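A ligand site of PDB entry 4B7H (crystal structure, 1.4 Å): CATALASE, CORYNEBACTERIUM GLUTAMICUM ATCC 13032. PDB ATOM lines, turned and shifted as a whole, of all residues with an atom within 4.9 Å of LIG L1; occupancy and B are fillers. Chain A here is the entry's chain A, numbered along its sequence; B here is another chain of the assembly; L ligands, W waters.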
ATOM      1  N   ARG A  67      29.938  22.589 -37.007  1.00  0.00           N
ATOM      2  CA  ARG A  67      29.990  23.560 -35.917  1.00  0.00           C
ATOM      3  C   ARG A  67      31.294  23.471 -35.144  1.00  0.00           C
ATOM      4  O   ARG A  67      31.821  22.371 -34.900  1.00  0.00           O
ATOM      5  CB  ARG A  67      28.876  23.280 -34.912  1.00  0.00           C
ATOM      6  CG  ARG A  67      27.489  23.505 -35.421  1.00  0.00           C
ATOM      7  CD  ARG A  67      26.531  22.700 -34.534  1.00  0.00           C
ATOM      8  NE  ARG A  67      25.140  22.998 -34.830  1.00  0.00           N
ATOM      9  CZ  ARG A  67      24.491  22.559 -35.907  1.00  0.00           C
ATOM     10  NH1 ARG A  67      25.111  21.770 -36.791  1.00  0.00           N
ATOM     11  NH2 ARG A  67      23.226  22.897 -36.090  1.00  0.00           N
ATOM     12  N   ILE A  68      31.794  24.626 -34.711  1.00  0.00           N
ATOM     13  CA  ILE A  68      32.827  24.661 -33.666  1.00  0.00           C
ATOM     14  C   ILE A  68      32.319  25.525 -32.507  1.00  0.00           C
ATOM     15  O   ILE A  68      32.008  26.709 -32.704  1.00  0.00           O
ATOM     16  CB  ILE A  68      34.195  25.168 -34.189  1.00  0.00           C
ATOM     17  CG1 ILE A  68      35.187  25.253 -33.022  1.00  0.00           C
ATOM     18  CG2 ILE A  68      34.089  26.505 -34.938  1.00  0.00           C
ATOM     19  CD1 ILE A  68      36.628  25.578 -33.441  1.00  0.00           C
ATOM     20  N   PRO A  69      32.153  24.933 -31.311  1.00  0.00           N
ATOM     21  CA  PRO A  69      32.184  23.508 -30.987  1.00  0.00           C
ATOM     22  C   PRO A  69      30.798  22.897 -31.199  1.00  0.00           C
ATOM     23  O   PRO A  69      29.991  23.477 -31.937  1.00  0.00           O
ATOM     24  CB  PRO A  69      32.574  23.509 -29.491  1.00  0.00           C
ATOM     25  CG  PRO A  69      32.242  24.912 -28.979  1.00  0.00           C
ATOM     26  CD  PRO A  69      31.731  25.726 -30.144  1.00  0.00           C
ATOM     27  N   HIS A  70      30.540  21.731 -30.588  1.00  0.00           N
ATOM     28  CA  HIS A  70      29.243  21.030 -30.653  1.00  0.00           C
ATOM     29  C   HIS A  70      28.968  20.447 -32.040  1.00  0.00           C
ATOM     30  O   HIS A  70      27.804  20.328 -32.450  1.00  0.00           O
ATOM     31  CB  HIS A  70      28.077  21.912 -30.192  1.00  0.00           C
ATOM     32  CG  HIS A  70      28.125  22.308 -28.744  1.00  0.00           C
ATOM     33  ND1 HIS A  70      27.361  21.689 -27.778  1.00  0.00           N
ATOM     34  CD2 HIS A  70      28.783  23.310 -28.106  1.00  0.00           C
ATOM     35  CE1 HIS A  70      27.567  22.275 -26.601  1.00  0.00           C
ATOM     36  NE2 HIS A  70      28.435  23.257 -26.781  1.00  0.00           N
ATOM     37  N   ARG A 106      18.229  20.410 -30.447  1.00  0.00           N
ATOM     38  CA  ARG A 106      19.423  19.681 -30.831  1.00  0.00           C
ATOM     39  C   ARG A 106      20.252  19.384 -29.581  1.00  0.00           C
ATOM     40  O   ARG A 106      20.479  20.284 -28.762  1.00  0.00           O
ATOM     41  CB  ARG A 106      20.242  20.445 -31.881  1.00  0.00           C
ATOM     42  CG  ARG A 106      21.450  19.660 -32.447  1.00  0.00           C
ATOM     43  CD  ARG A 106      22.119  20.441 -33.569  1.00  0.00           C
ATOM     44  NE  ARG A 106      23.299  19.774 -34.131  1.00  0.00           N
ATOM     45  CZ  ARG A 106      24.522  19.832 -33.613  1.00  0.00           C
ATOM     46  NH1 ARG A 106      24.741  20.504 -32.482  1.00  0.00           N
ATOM     47  NH2 ARG A 106      25.538  19.200 -34.215  1.00  0.00           N
ATOM     48  N   SER A 108      23.954  17.460 -28.209  1.00  0.00           N
ATOM     49  CA  SER A 108      25.290  17.347 -28.777  1.00  0.00           C
ATOM     50  C   SER A 108      26.332  17.068 -27.714  1.00  0.00           C
ATOM     51  O   SER A 108      26.060  17.196 -26.531  1.00  0.00           O
ATOM     52  CB  SER A 108      25.653  18.665 -29.491  1.00  0.00           C
ATOM     53  OG  SER A 108      25.519  19.759 -28.599  1.00  0.00           O
ATOM     54  N   GLY A 125      25.228  19.503 -25.089  1.00  0.00           N
ATOM     55  CA  GLY A 125      24.379  20.603 -25.467  1.00  0.00           C
ATOM     56  C   GLY A 125      22.914  20.217 -25.391  1.00  0.00           C
ATOM     57  O   GLY A 125      22.537  19.076 -25.621  1.00  0.00           O
ATOM     58  N   PHE A 126      22.085  21.217 -25.081  1.00  0.00           N
ATOM     59  CA  PHE A 126      20.647  21.025 -24.867  1.00  0.00           C
ATOM     60  C   PHE A 126      20.013  22.312 -25.405  1.00  0.00           C
ATOM     61  O   PHE A 126      19.709  23.243 -24.651  1.00  0.00           O
ATOM     62  CB  PHE A 126      20.400  20.862 -23.355  1.00  0.00           C
ATOM     63  CG  PHE A 126      19.075  20.249 -22.996  1.00  0.00           C
ATOM     64  CD1 PHE A 126      17.890  20.922 -23.255  1.00  0.00           C
ATOM     65  CD2 PHE A 126      19.011  19.020 -22.345  1.00  0.00           C
ATOM     66  CE1 PHE A 126      16.657  20.372 -22.902  1.00  0.00           C
ATOM     67  CE2 PHE A 126      17.773  18.461 -21.983  1.00  0.00           C
ATOM     68  CZ  PHE A 126      16.602  19.139 -22.261  1.00  0.00           C
ATOM     69  N   ALA A 127      19.819  22.354 -26.726  1.00  0.00           N
ATOM     70  CA  ALA A 127      19.499  23.590 -27.412  1.00  0.00           C
ATOM     71  C   ALA A 127      18.100  23.586 -28.011  1.00  0.00           C
ATOM     72  O   ALA A 127      17.817  22.815 -28.946  1.00  0.00           O
ATOM     73  CB  ALA A 127      20.537  23.858 -28.499  1.00  0.00           C
ATOM     74  N   VAL A 140      19.527  28.170 -25.839  1.00  0.00           N
ATOM     75  CA  VAL A 140      20.631  27.320 -26.239  1.00  0.00           C
ATOM     76  C   VAL A 140      21.382  26.963 -24.962  1.00  0.00           C
ATOM     77  O   VAL A 140      22.295  27.685 -24.522  1.00  0.00           O
ATOM     78  CB  VAL A 140      21.516  28.036 -27.280  1.00  0.00           C
ATOM     79  CG1 VAL A 140      22.641  27.122 -27.762  1.00  0.00           C
ATOM     80  CG2 VAL A 140      20.661  28.493 -28.474  1.00  0.00           C
ATOM     81  N   GLY A 141      20.948  25.870 -24.341  1.00  0.00           N
ATOM     82  CA  GLY A 141      21.470  25.490 -23.048  1.00  0.00           C
ATOM     83  C   GLY A 141      22.400  24.296 -23.084  1.00  0.00           C
ATOM     84  O   GLY A 141      22.793  23.845 -24.157  1.00  0.00           O
ATOM     85  N   ASN A 142      22.757  23.805 -21.907  1.00  0.00           N
ATOM     86  CA  ASN A 142      23.587  22.611 -21.734  1.00  0.00           C
ATOM     87  C   ASN A 142      22.968  21.736 -20.656  1.00  0.00           C
ATOM     88  O   ASN A 142      22.024  22.165 -19.980  1.00  0.00           O
ATOM     89  CB  ASN A 142      25.011  22.997 -21.310  1.00  0.00           C
ATOM     90  CG  ASN A 142      25.928  23.336 -22.476  1.00  0.00           C
ATOM     91  OD1 ASN A 142      25.794  22.799 -23.580  1.00  0.00           O
ATOM     92  ND2 ASN A 142      26.889  24.212 -22.219  1.00  0.00           N
ATOM     93  N   PHE A 147      29.188  26.637 -16.088  1.00  0.00           N
ATOM     94  CA  PHE A 147      30.131  26.422 -17.186  1.00  0.00           C
ATOM     95  C   PHE A 147      31.536  26.770 -16.714  1.00  0.00           C
ATOM     96  O   PHE A 147      31.720  27.233 -15.582  1.00  0.00           O
ATOM     97  CB  PHE A 147      29.739  27.265 -18.398  1.00  0.00           C
ATOM     98  CG  PHE A 147      30.298  26.745 -19.713  1.00  0.00           C
ATOM     99  CD1 PHE A 147      29.885  25.523 -20.217  1.00  0.00           C
ATOM    100  CD2 PHE A 147      31.181  27.516 -20.452  1.00  0.00           C
ATOM    101  CE1 PHE A 147      30.377  25.047 -21.441  1.00  0.00           C
ATOM    102  CE2 PHE A 147      31.678  27.049 -21.675  1.00  0.00           C
ATOM    103  CZ  PHE A 147      31.265  25.826 -22.169  1.00  0.00           C
ATOM    104  N   GLY A 152      33.984  35.670 -22.144  1.00  0.00           N
ATOM    105  CA  GLY A 152      34.059  35.144 -23.496  1.00  0.00           C
ATOM    106  C   GLY A 152      35.432  35.265 -24.134  1.00  0.00           C
ATOM    107  O   GLY A 152      35.745  34.520 -25.060  1.00  0.00           O
ATOM    108  N   PHE A 155      36.998  31.881 -24.108  1.00  0.00           N
ATOM    109  CA  PHE A 155      36.307  30.735 -24.683  1.00  0.00           C
ATOM    110  C   PHE A 155      37.101  29.996 -25.773  1.00  0.00           C
ATOM    111  O   PHE A 155      37.201  28.763 -25.720  1.00  0.00           O
ATOM    112  CB  PHE A 155      34.895  31.142 -25.125  1.00  0.00           C
ATOM    113  CG  PHE A 155      34.123  30.056 -25.798  1.00  0.00           C
ATOM    114  CD1 PHE A 155      33.503  29.060 -25.065  1.00  0.00           C
ATOM    115  CD2 PHE A 155      33.999  30.040 -27.182  1.00  0.00           C
ATOM    116  CE1 PHE A 155      32.769  28.065 -25.694  1.00  0.00           C
ATOM    117  CE2 PHE A 155      33.270  29.054 -27.811  1.00  0.00           C
ATOM    118  CZ  PHE A 155      32.646  28.071 -27.067  1.00  0.00           C
ATOM    119  N   PHE A 209      19.557  23.036 -18.916  1.00  0.00           N
ATOM    120  CA  PHE A 209      19.588  24.309 -18.184  1.00  0.00           C
ATOM    121  C   PHE A 209      19.911  25.432 -19.137  1.00  0.00           C
ATOM    122  O   PHE A 209      20.665  25.222 -20.086  1.00  0.00           O
ATOM    123  CB  PHE A 209      20.700  24.300 -17.120  1.00  0.00           C
ATOM    124  CG  PHE A 209      20.622  23.144 -16.156  1.00  0.00           C
ATOM    125  CD1 PHE A 209      21.224  21.938 -16.466  1.00  0.00           C
ATOM    126  CD2 PHE A 209      19.987  23.276 -14.928  1.00  0.00           C
ATOM    127  CE1 PHE A 209      21.177  20.861 -15.589  1.00  0.00           C
ATOM    128  CE2 PHE A 209      19.936  22.212 -14.030  1.00  0.00           C
ATOM    129  CZ  PHE A 209      20.533  20.997 -14.360  1.00  0.00           C
ATOM    130  N   GLY A 210      19.367  26.621 -18.896  1.00  0.00           N
ATOM    131  CA  GLY A 210      19.810  27.794 -19.635  1.00  0.00           C
ATOM    132  C   GLY A 210      21.196  28.234 -19.189  1.00  0.00           C
ATOM    133  O   GLY A 210      21.907  28.939 -19.913  1.00  0.00           O
ATOM    134  N   SER A 211      21.556  27.809 -17.981  1.00  0.00           N
ATOM    135  CA  SER A 211      22.826  28.119 -17.301  1.00  0.00           C
ATOM    136  C   SER A 211      22.963  29.589 -16.891  1.00  0.00           C
ATOM    137  O   SER A 211      23.082  29.890 -15.697  1.00  0.00           O
ATOM    138  CB  SER A 211      24.057  27.652 -18.095  1.00  0.00           C
ATOM    139  OG  SER A 211      23.926  26.318 -18.560  1.00  0.00           O
ATOM    140  N   HIS A 212      22.951  30.497 -17.866  1.00  0.00           N
ATOM    141  CA  HIS A 212      23.043  31.928 -17.568  1.00  0.00           C
ATOM    142  C   HIS A 212      21.824  32.461 -16.842  1.00  0.00           C
ATOM    143  O   HIS A 212      20.719  31.944 -16.996  1.00  0.00           O
ATOM    144  CB  HIS A 212      23.117  32.792 -18.844  1.00  0.00           C
ATOM    145  CG  HIS A 212      24.155  32.371 -19.828  1.00  0.00           C
ATOM    146  ND1 HIS A 212      25.498  32.654 -19.660  1.00  0.00           N
ATOM    147  CD2 HIS A 212      24.063  31.724 -21.016  1.00  0.00           C
ATOM    148  CE1 HIS A 212      26.181  32.190 -20.690  1.00  0.00           C
ATOM    149  NE2 HIS A 212      25.327  31.625 -21.534  1.00  0.00           N
ATOM    150  N   LEU A 293      28.557  33.177 -14.496  1.00  0.00           N
ATOM    151  CA  LEU A 293      28.137  31.878 -14.993  1.00  0.00           C
ATOM    152  C   LEU A 293      28.687  30.705 -14.192  1.00  0.00           C
ATOM    153  O   LEU A 293      28.036  29.642 -14.102  1.00  0.00           O
ATOM    154  CB  LEU A 293      28.525  31.757 -16.474  1.00  0.00           C
ATOM    155  CG  LEU A 293      28.192  30.456 -17.211  1.00  0.00           C
ATOM    156  CD1 LEU A 293      26.681  30.175 -17.171  1.00  0.00           C
ATOM    157  CD2 LEU A 293      28.713  30.556 -18.631  1.00  0.00           C
ATOM    158  N   ILE A 326      20.146  23.586 -38.844  1.00  0.00           N
ATOM    159  CA  ILE A 326      19.484  24.463 -37.877  1.00  0.00           C
ATOM    160  C   ILE A 326      20.535  25.435 -37.314  1.00  0.00           C
ATOM    161  O   ILE A 326      21.716  25.090 -37.203  1.00  0.00           O
ATOM    162  CB  ILE A 326      18.725  23.686 -36.766  1.00  0.00           C
ATOM    163  CG1 ILE A 326      17.620  24.573 -36.175  1.00  0.00           C
ATOM    164  CG2 ILE A 326      19.665  23.176 -35.664  1.00  0.00           C
ATOM    165  CD1 ILE A 326      16.646  23.821 -35.276  1.00  0.00           C
ATOM    166  N   ALA A 327      20.091  26.659 -37.041  1.00  0.00           N
ATOM    167  CA  ALA A 327      20.999  27.704 -36.588  1.00  0.00           C
ATOM    168  C   ALA A 327      20.493  28.193 -35.244  1.00  0.00           C
ATOM    169  O   ALA A 327      19.778  29.198 -35.153  1.00  0.00           O
ATOM    170  CB  ALA A 327      21.037  28.850 -37.603  1.00  0.00           C
ATOM    171  N   LEU A 328      20.815  27.454 -34.188  1.00  0.00           N
ATOM    172  CA  LEU A 328      20.316  27.790 -32.850  1.00  0.00           C
ATOM    173  C   LEU A 328      21.185  28.908 -32.274  1.00  0.00           C
ATOM    174  O   LEU A 328      22.407  28.871 -32.410  1.00  0.00           O
ATOM    175  CB  LEU A 328      20.303  26.547 -31.979  1.00  0.00           C
ATOM    176  CG  LEU A 328      19.240  25.531 -32.443  1.00  0.00           C
ATOM    177  CD1 LEU A 328      19.542  24.099 -31.985  1.00  0.00           C
ATOM    178  CD2 LEU A 328      17.845  25.932 -31.974  1.00  0.00           C
ATOM    179  N   MET A 344      29.885  36.052 -20.530  1.00  0.00           N
ATOM    180  CA  MET A 344      29.846  34.893 -21.427  1.00  0.00           C
ATOM    181  C   MET A 344      28.621  35.003 -22.329  1.00  0.00           C
ATOM    182  O   MET A 344      28.729  34.887 -23.554  1.00  0.00           O
ATOM    183  CB  MET A 344      29.828  33.599 -20.618  1.00  0.00           C
ATOM    184  CG  MET A 344      31.129  33.318 -19.872  1.00  0.00           C
ATOM    185  SD  MET A 344      32.431  32.652 -20.913  1.00  0.00           S
ATOM    186  CE  MET A 344      31.840  30.973 -21.037  1.00  0.00           C
ATOM    187  N   ALA A 347      29.024  37.738 -25.018  1.00  0.00           N
ATOM    188  CA  ALA A 347      29.829  37.269 -26.147  1.00  0.00           C
ATOM    189  C   ALA A 347      29.050  36.300 -27.036  1.00  0.00           C
ATOM    190  O   ALA A 347      29.126  36.396 -28.273  1.00  0.00           O
ATOM    191  CB  ALA A 347      31.124  36.627 -25.646  1.00  0.00           C
ATOM    192  N   ARG A 348      28.301  35.382 -26.442  1.00  0.00           N
ATOM    193  CA  ARG A 348      27.472  34.445 -27.200  1.00  0.00           C
ATOM    194  C   ARG A 348      26.467  35.164 -28.105  1.00  0.00           C
ATOM    195  O   ARG A 348      26.212  34.717 -29.217  1.00  0.00           O
ATOM    196  CB  ARG A 348      26.732  33.495 -26.276  1.00  0.00           C
ATOM    197  CG  ARG A 348      27.632  32.565 -25.491  1.00  0.00           C
ATOM    198  CD  ARG A 348      26.804  31.665 -24.597  1.00  0.00           C
ATOM    199  NE  ARG A 348      26.111  30.643 -25.367  1.00  0.00           N
ATOM    200  CZ  ARG A 348      24.932  30.110 -25.042  1.00  0.00           C
ATOM    201  NH1 ARG A 348      24.295  30.511 -23.944  1.00  0.00           N
ATOM    202  NH2 ARG A 348      24.390  29.177 -25.827  1.00  0.00           N
ATOM    203  N   ALA A 351      28.380  35.728 -31.131  1.00  0.00           N
ATOM    204  CA  ALA A 351      29.143  34.655 -31.775  1.00  0.00           C
ATOM    205  C   ALA A 351      28.359  33.676 -32.644  1.00  0.00           C
ATOM    206  O   ALA A 351      28.893  33.189 -33.637  1.00  0.00           O
ATOM    207  CB  ALA A 351      29.935  33.898 -30.734  1.00  0.00           C
ATOM    208  N   TYR A 352      27.121  33.368 -32.282  1.00  0.00           N
ATOM    209  CA  TYR A 352      26.416  32.280 -32.974  1.00  0.00           C
ATOM    210  C   TYR A 352      26.012  32.670 -34.385  1.00  0.00           C
ATOM    211  O   TYR A 352      26.313  31.945 -35.341  1.00  0.00           O
ATOM    212  CB  TYR A 352      25.210  31.775 -32.179  1.00  0.00           C
ATOM    213  CG  TYR A 352      25.592  31.016 -30.933  1.00  0.00           C
ATOM    214  CD1 TYR A 352      26.302  31.628 -29.899  1.00  0.00           C
ATOM    215  CD2 TYR A 352      25.239  29.683 -30.770  1.00  0.00           C
ATOM    216  CE1 TYR A 352      26.661  30.933 -28.761  1.00  0.00           C
ATOM    217  CE2 TYR A 352      25.580  28.975 -29.623  1.00  0.00           C
ATOM    218  CZ  TYR A 352      26.305  29.615 -28.628  1.00  0.00           C
ATOM    219  OH  TYR A 352      26.637  28.934 -27.480  1.00  0.00           O
ATOM    220  N   GLN A 355      29.033  32.829 -36.623  1.00  0.00           N
ATOM    221  CA  GLN A 355      29.469  31.554 -37.168  1.00  0.00           C
ATOM    222  C   GLN A 355      28.481  31.038 -38.232  1.00  0.00           C
ATOM    223  O   GLN A 355      28.884  30.500 -39.269  1.00  0.00           O
ATOM    224  CB  GLN A 355      29.680  30.486 -36.097  1.00  0.00           C
ATOM    225  CG  GLN A 355      30.197  29.194 -36.752  1.00  0.00           C
ATOM    226  CD  GLN A 355      30.737  28.145 -35.796  1.00  0.00           C
ATOM    227  OE1 GLN A 355      30.717  26.949 -36.114  1.00  0.00           O
ATOM    228  NE2 GLN A 355      31.255  28.572 -34.641  1.00  0.00           N
ATOM    229  N   GLN A 356      27.192  31.220 -37.981  1.00  0.00           N
ATOM    230  CA  GLN A 356      26.171  30.704 -38.885  1.00  0.00           C
ATOM    231  C   GLN A 356      26.202  31.367 -40.250  1.00  0.00           C
ATOM    232  O   GLN A 356      25.983  30.713 -41.269  1.00  0.00           O
ATOM    233  CB  GLN A 356      24.793  30.801 -38.208  1.00  0.00           C
ATOM    234  CG  GLN A 356      24.669  29.766 -37.090  1.00  0.00           C
ATOM    235  CD  GLN A 356      23.751  30.195 -35.964  1.00  0.00           C
ATOM    236  OE1 GLN A 356      23.112  31.256 -36.010  1.00  0.00           O
ATOM    237  NE2 GLN A 356      23.671  29.346 -34.937  1.00  0.00           N
ATOM    238  N   ARG A 359      29.129  29.301 -41.656  1.00  0.00           N
ATOM    239  CA  ARG A 359      28.930  27.858 -41.665  1.00  0.00           C
ATOM    240  C   ARG A 359      27.834  27.455 -42.646  1.00  0.00           C
ATOM    241  O   ARG A 359      27.936  26.426 -43.316  1.00  0.00           O
ATOM    242  CB  ARG A 359      28.566  27.420 -40.236  1.00  0.00           C
ATOM    243  CG  ARG A 359      28.205  25.970 -40.128  1.00  0.00           C
ATOM    244  CD  ARG A 359      28.074  25.540 -38.686  1.00  0.00           C
ATOM    245  NE  ARG A 359      26.861  25.979 -37.983  1.00  0.00           N
ATOM    246  CZ  ARG A 359      25.648  25.454 -38.159  1.00  0.00           C
ATOM    247  NH1 ARG A 359      25.444  24.537 -39.089  1.00  0.00           N
ATOM    248  NH2 ARG A 359      24.640  25.892 -37.404  1.00  0.00           N
ATOM    249  N   LEU B  56      37.080  35.854 -31.446  1.00  0.00           N
ATOM    250  CA  LEU B  56      35.866  35.056 -31.613  1.00  0.00           C
ATOM    251  C   LEU B  56      35.545  34.788 -33.099  1.00  0.00           C
ATOM    252  O   LEU B  56      35.148  33.675 -33.459  1.00  0.00           O
ATOM    253  CB  LEU B  56      34.666  35.729 -30.941  1.00  0.00           C
ATOM    254  CG  LEU B  56      34.694  35.837 -29.425  1.00  0.00           C
ATOM    255  CD1 LEU B  56      33.499  36.665 -28.957  1.00  0.00           C
ATOM    256  CD2 LEU B  56      34.683  34.454 -28.779  1.00  0.00           C
ATOM    257  N   ASN B  60      35.368  31.252 -35.013  1.00  0.00           N
ATOM    258  CA  ASN B  60      34.134  30.842 -35.686  1.00  0.00           C
ATOM    259  C   ASN B  60      34.348  30.300 -37.096  1.00  0.00           C
ATOM    260  O   ASN B  60      33.461  29.648 -37.643  1.00  0.00           O
ATOM    261  CB  ASN B  60      33.141  32.008 -35.772  1.00  0.00           C
ATOM    262  CG  ASN B  60      32.366  32.236 -34.482  1.00  0.00           C
ATOM    263  OD1 ASN B  60      31.805  33.332 -34.255  1.00  0.00           O
ATOM    264  ND2 ASN B  60      32.308  31.223 -33.632  1.00  0.00           N
HETATM  265  C1  LIG L   1      27.519  25.947 -30.119  1.00  0.00           C
HETATM  266  C2  LIG L   1      29.912  30.044 -29.095  1.00  0.00           C
HETATM  267  C3  LIG L   1      29.366  29.095 -24.376  1.00  0.00           C
HETATM  268  C4  LIG L   1      25.842  26.037 -25.533  1.00  0.00           C
HETATM  269  C5  LIG L   1      28.219  27.122 -30.254  1.00  0.00           C
HETATM  270  C6  LIG L   1      28.580  27.759 -31.505  1.00  0.00           C
HETATM  271  C7  LIG L   1      29.220  28.901 -31.211  1.00  0.00           C
HETATM  272  C8  LIG L   1      29.307  29.014 -29.774  1.00  0.00           C
HETATM  273  C9  LIG L   1      29.795  29.943 -32.173  1.00  0.00           C
HETATM  274  C10 LIG L   1      28.238  27.201 -32.913  1.00  0.00           C
HETATM  275  C11 LIG L   1      26.861  27.691 -33.321  1.00  0.00           C
HETATM  276  C12 LIG L   1      26.528  27.358 -34.750  1.00  0.00           C
HETATM  277  O1  LIG L   1      25.333  27.032 -34.998  1.00  0.00           O
HETATM  278  O2  LIG L   1      27.404  27.410 -35.647  1.00  0.00           O
HETATM  279  C13 LIG L   1      30.003  30.147 -27.729  1.00  0.00           C
HETATM  280  C14 LIG L   1      30.719  31.169 -26.999  1.00  0.00           C
HETATM  281  C15 LIG L   1      30.586  30.884 -25.680  1.00  0.00           C
HETATM  282  C16 LIG L   1      29.765  29.697 -25.568  1.00  0.00           C
HETATM  283  C17 LIG L   1      31.491  32.318 -27.664  1.00  0.00           C
HETATM  284  C18 LIG L   1      31.111  31.634 -24.443  1.00  0.00           C
HETATM  285  C19 LIG L   1      31.341  32.947 -24.458  1.00  0.00           C
HETATM  286  C20 LIG L   1      28.243  28.314 -24.271  1.00  0.00           C
HETATM  287  C21 LIG L   1      27.390  28.134 -23.098  1.00  0.00           C
HETATM  288  C22 LIG L   1      26.403  27.276 -23.445  1.00  0.00           C
HETATM  289  C23 LIG L   1      26.615  26.916 -24.828  1.00  0.00           C
HETATM  290  C24 LIG L   1      27.616  28.814 -21.727  1.00  0.00           C
HETATM  291  C25 LIG L   1      25.197  26.769 -22.629  1.00  0.00           C
HETATM  292  C26 LIG L   1      24.632  27.490 -21.647  1.00  0.00           C
HETATM  293  C27 LIG L   1      26.027  25.689 -26.845  1.00  0.00           C
HETATM  294  C28 LIG L   1      25.252  24.683 -27.496  1.00  0.00           C
HETATM  295  C29 LIG L   1      25.755  24.645 -28.912  1.00  0.00           C
HETATM  296  C30 LIG L   1      26.792  25.643 -28.999  1.00  0.00           C
HETATM  297  C31 LIG L   1      24.156  23.817 -26.883  1.00  0.00           C
HETATM  298  C32 LIG L   1      25.222  23.732 -30.006  1.00  0.00           C
HETATM  299  C33 LIG L   1      23.907  24.317 -30.510  1.00  0.00           C
HETATM  300  C34 LIG L   1      23.379  23.330 -31.517  1.00  0.00           C
HETATM  301  O3  LIG L   1      23.298  23.659 -32.726  1.00  0.00           O
HETATM  302  O4  LIG L   1      23.071  22.178 -31.106  1.00  0.00           O
HETATM  303  N1  LIG L   1      28.677  27.918 -29.205  1.00  0.00           N
HETATM  304  N2  LIG L   1      29.436  29.263 -26.830  1.00  0.00           N
HETATM  305  N3  LIG L   1      27.724  27.551 -25.309  1.00  0.00           N
HETATM  306  N4  LIG L   1      26.935  26.237 -27.743  1.00  0.00           N
HETATM  307 FE1  LIG L   1      28.221  27.700 -27.258  1.00  0.00          FE
HETATM  308  N1  LG2 L   2      29.483  26.605 -26.945  1.00  0.00           N
HETATM  309  O1  LG2 L   2      30.272  26.142 -26.303  1.00  0.00           O
HETATM  310  O   HOH W   1      28.931  24.558 -24.301  1.00  0.00           O
HETATM  311  O   HOH W   2      26.567  25.764 -19.639  1.00  0.00           O
HETATM  312  O   HOH W   3      23.158  20.947 -28.732  1.00  0.00           O
HETATM  313  O   HOH W   4      23.046  25.723 -34.348  1.00  0.00           O
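An iron atom (FE1) of LIG L1 is bound by the side-chain hydroxyl (OH) of Tyr 352, at 2.0 Å.
O1 of LG2 L2 sits at hydrogen-bond distance from NE2 of His 70.
The side-chain amide nitrogen of Gln 356 lies within hydrogen-bond range of an oxygen (O1) of LIG L1 (2.8 Å).
NE of Arg 67 is in salt-bridge range of O3 of LIG L1, at 2.9 Å.
NH1 of Arg 106 is in salt-bridge range of O4 of LIG L1, 2.7 Å away.
OE1 of Gln 355 lies close to O2 of LIG L1, at 3.4 Å.
The guanidinium group of Arg 359 lies within salt-bridge range of an oxygen (O1) of LIG L1.
An iron atom (FE1) of LIG L1 is bound by a nitrogen (N1) of LG2 L2 (1.7 Å).
The backbone NH (N) of Gly 152 is in hydrogen-bond range of the side-chain sulfur (SD) of Met 344, at 3.6 Å.
O of Tyr 352 lies close to OE1 of Gln 356, 3.3 Å away.
The backbone carbonyl oxygen (O) of Leu 56 of chain B sits close to the side-chain amide oxygen (OD1) of Asn 60 of chain B.
O of Ile 326 lies within hydrogen-bond range of NH2 of Arg 359, 3.0 Å away.
ND2 of Asn 60 of chain B sits close to NE2 of Gln 355, 3.0 Å away.
OG of Ser 108 is in hydrogen-bond range of ND1 of His 70 (2.8 Å).
The backbone carbonyl oxygen (O) of Ala 127 is in hydrogen-bond range of the backbone NH (N) of Arg 106 (2.9 Å).
NH1 of Arg 348 is in hydrogen-bond range of NE2 of His 212, 2.8 Å away.
A ring nitrogen (NE2) of His 70 lies close to a nitrogen (N4) of LIG L1, 3.5 Å away.
NE of Arg 348 sits close to N3 of LIG L1 (3.5 Å).
Merely in contact with LIG L1: Ile 68 (3.8 Å), Pro 69 (3.8 Å), Gly 125 (3.5 Å), Phe 126 (3.8 Å), Ala 127 (3.95 Å), Val 140 (3.6 Å), Gly 141 (3.0 Å), Asn 142 (3.1 Å), Phe 147 (3.9 Å), Gly 152 (3.6 Å), Phe 155 (3.4 Å), Gly 210 (3.5 Å), Ser 211 (3.4 Å), His 212 (3.6 Å), Leu 293 (3.7 Å), Leu 328 (3.9 Å), Met 344 (3.4 Å), Ala 347 (3.9 Å), Ala 351 (3.7 Å), Leu 56 of chain B (3.999 Å) and Asn 60 of chain B (3.2 Å).
Hydrophobic or aromatic side chains that line LIG L1: Pro 69, His 70, Ala 127, Val 140, Phe 147, Phe 155, His 212, Leu 293, Leu 328, Met 344, Ala 347, Ala 351, Tyr 352 and Leu 56 of chain B.
29 residues have an atom within 4 Å of LIG L1: Arg 67, Ile 68, Pro 69, His 70, Arg 106, Gly 125, Phe 126, Ala 127, Val 140, Gly 141, Asn 142, Phe 147, Gly 152, Phe 155, Gly 210, Ser 211, His 212, Leu 293, Leu 328, Met 344, Ala 347, Arg 348, Ala 351, Tyr 352, Gln 355, Gln 356, Arg 359, Leu 56 of chain B and Asn 60 of chain B.
The nearest printed residue that does not touch LIG L1 is Ser 108 (4.2 Å).
Water W3 lies within hydrogen-bond range of OG of Ser 108 (2.6 Å), O4 of LIG L1 (2.7 Å) and O of Arg 106 (2.8 Å).
Water W2 bridges the side-chain hydroxyl (OG) of Ser 211 and the side-chain amide nitrogen (ND2) of Asn 142.
Water W1 lies within hydrogen-bond range of a ring nitrogen (NE2) of His 70 (2.8 Å), an oxygen (O1) of LG2 L2 (2.9 Å) and the side-chain amide nitrogen of Asn 142 (2.9 Å).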
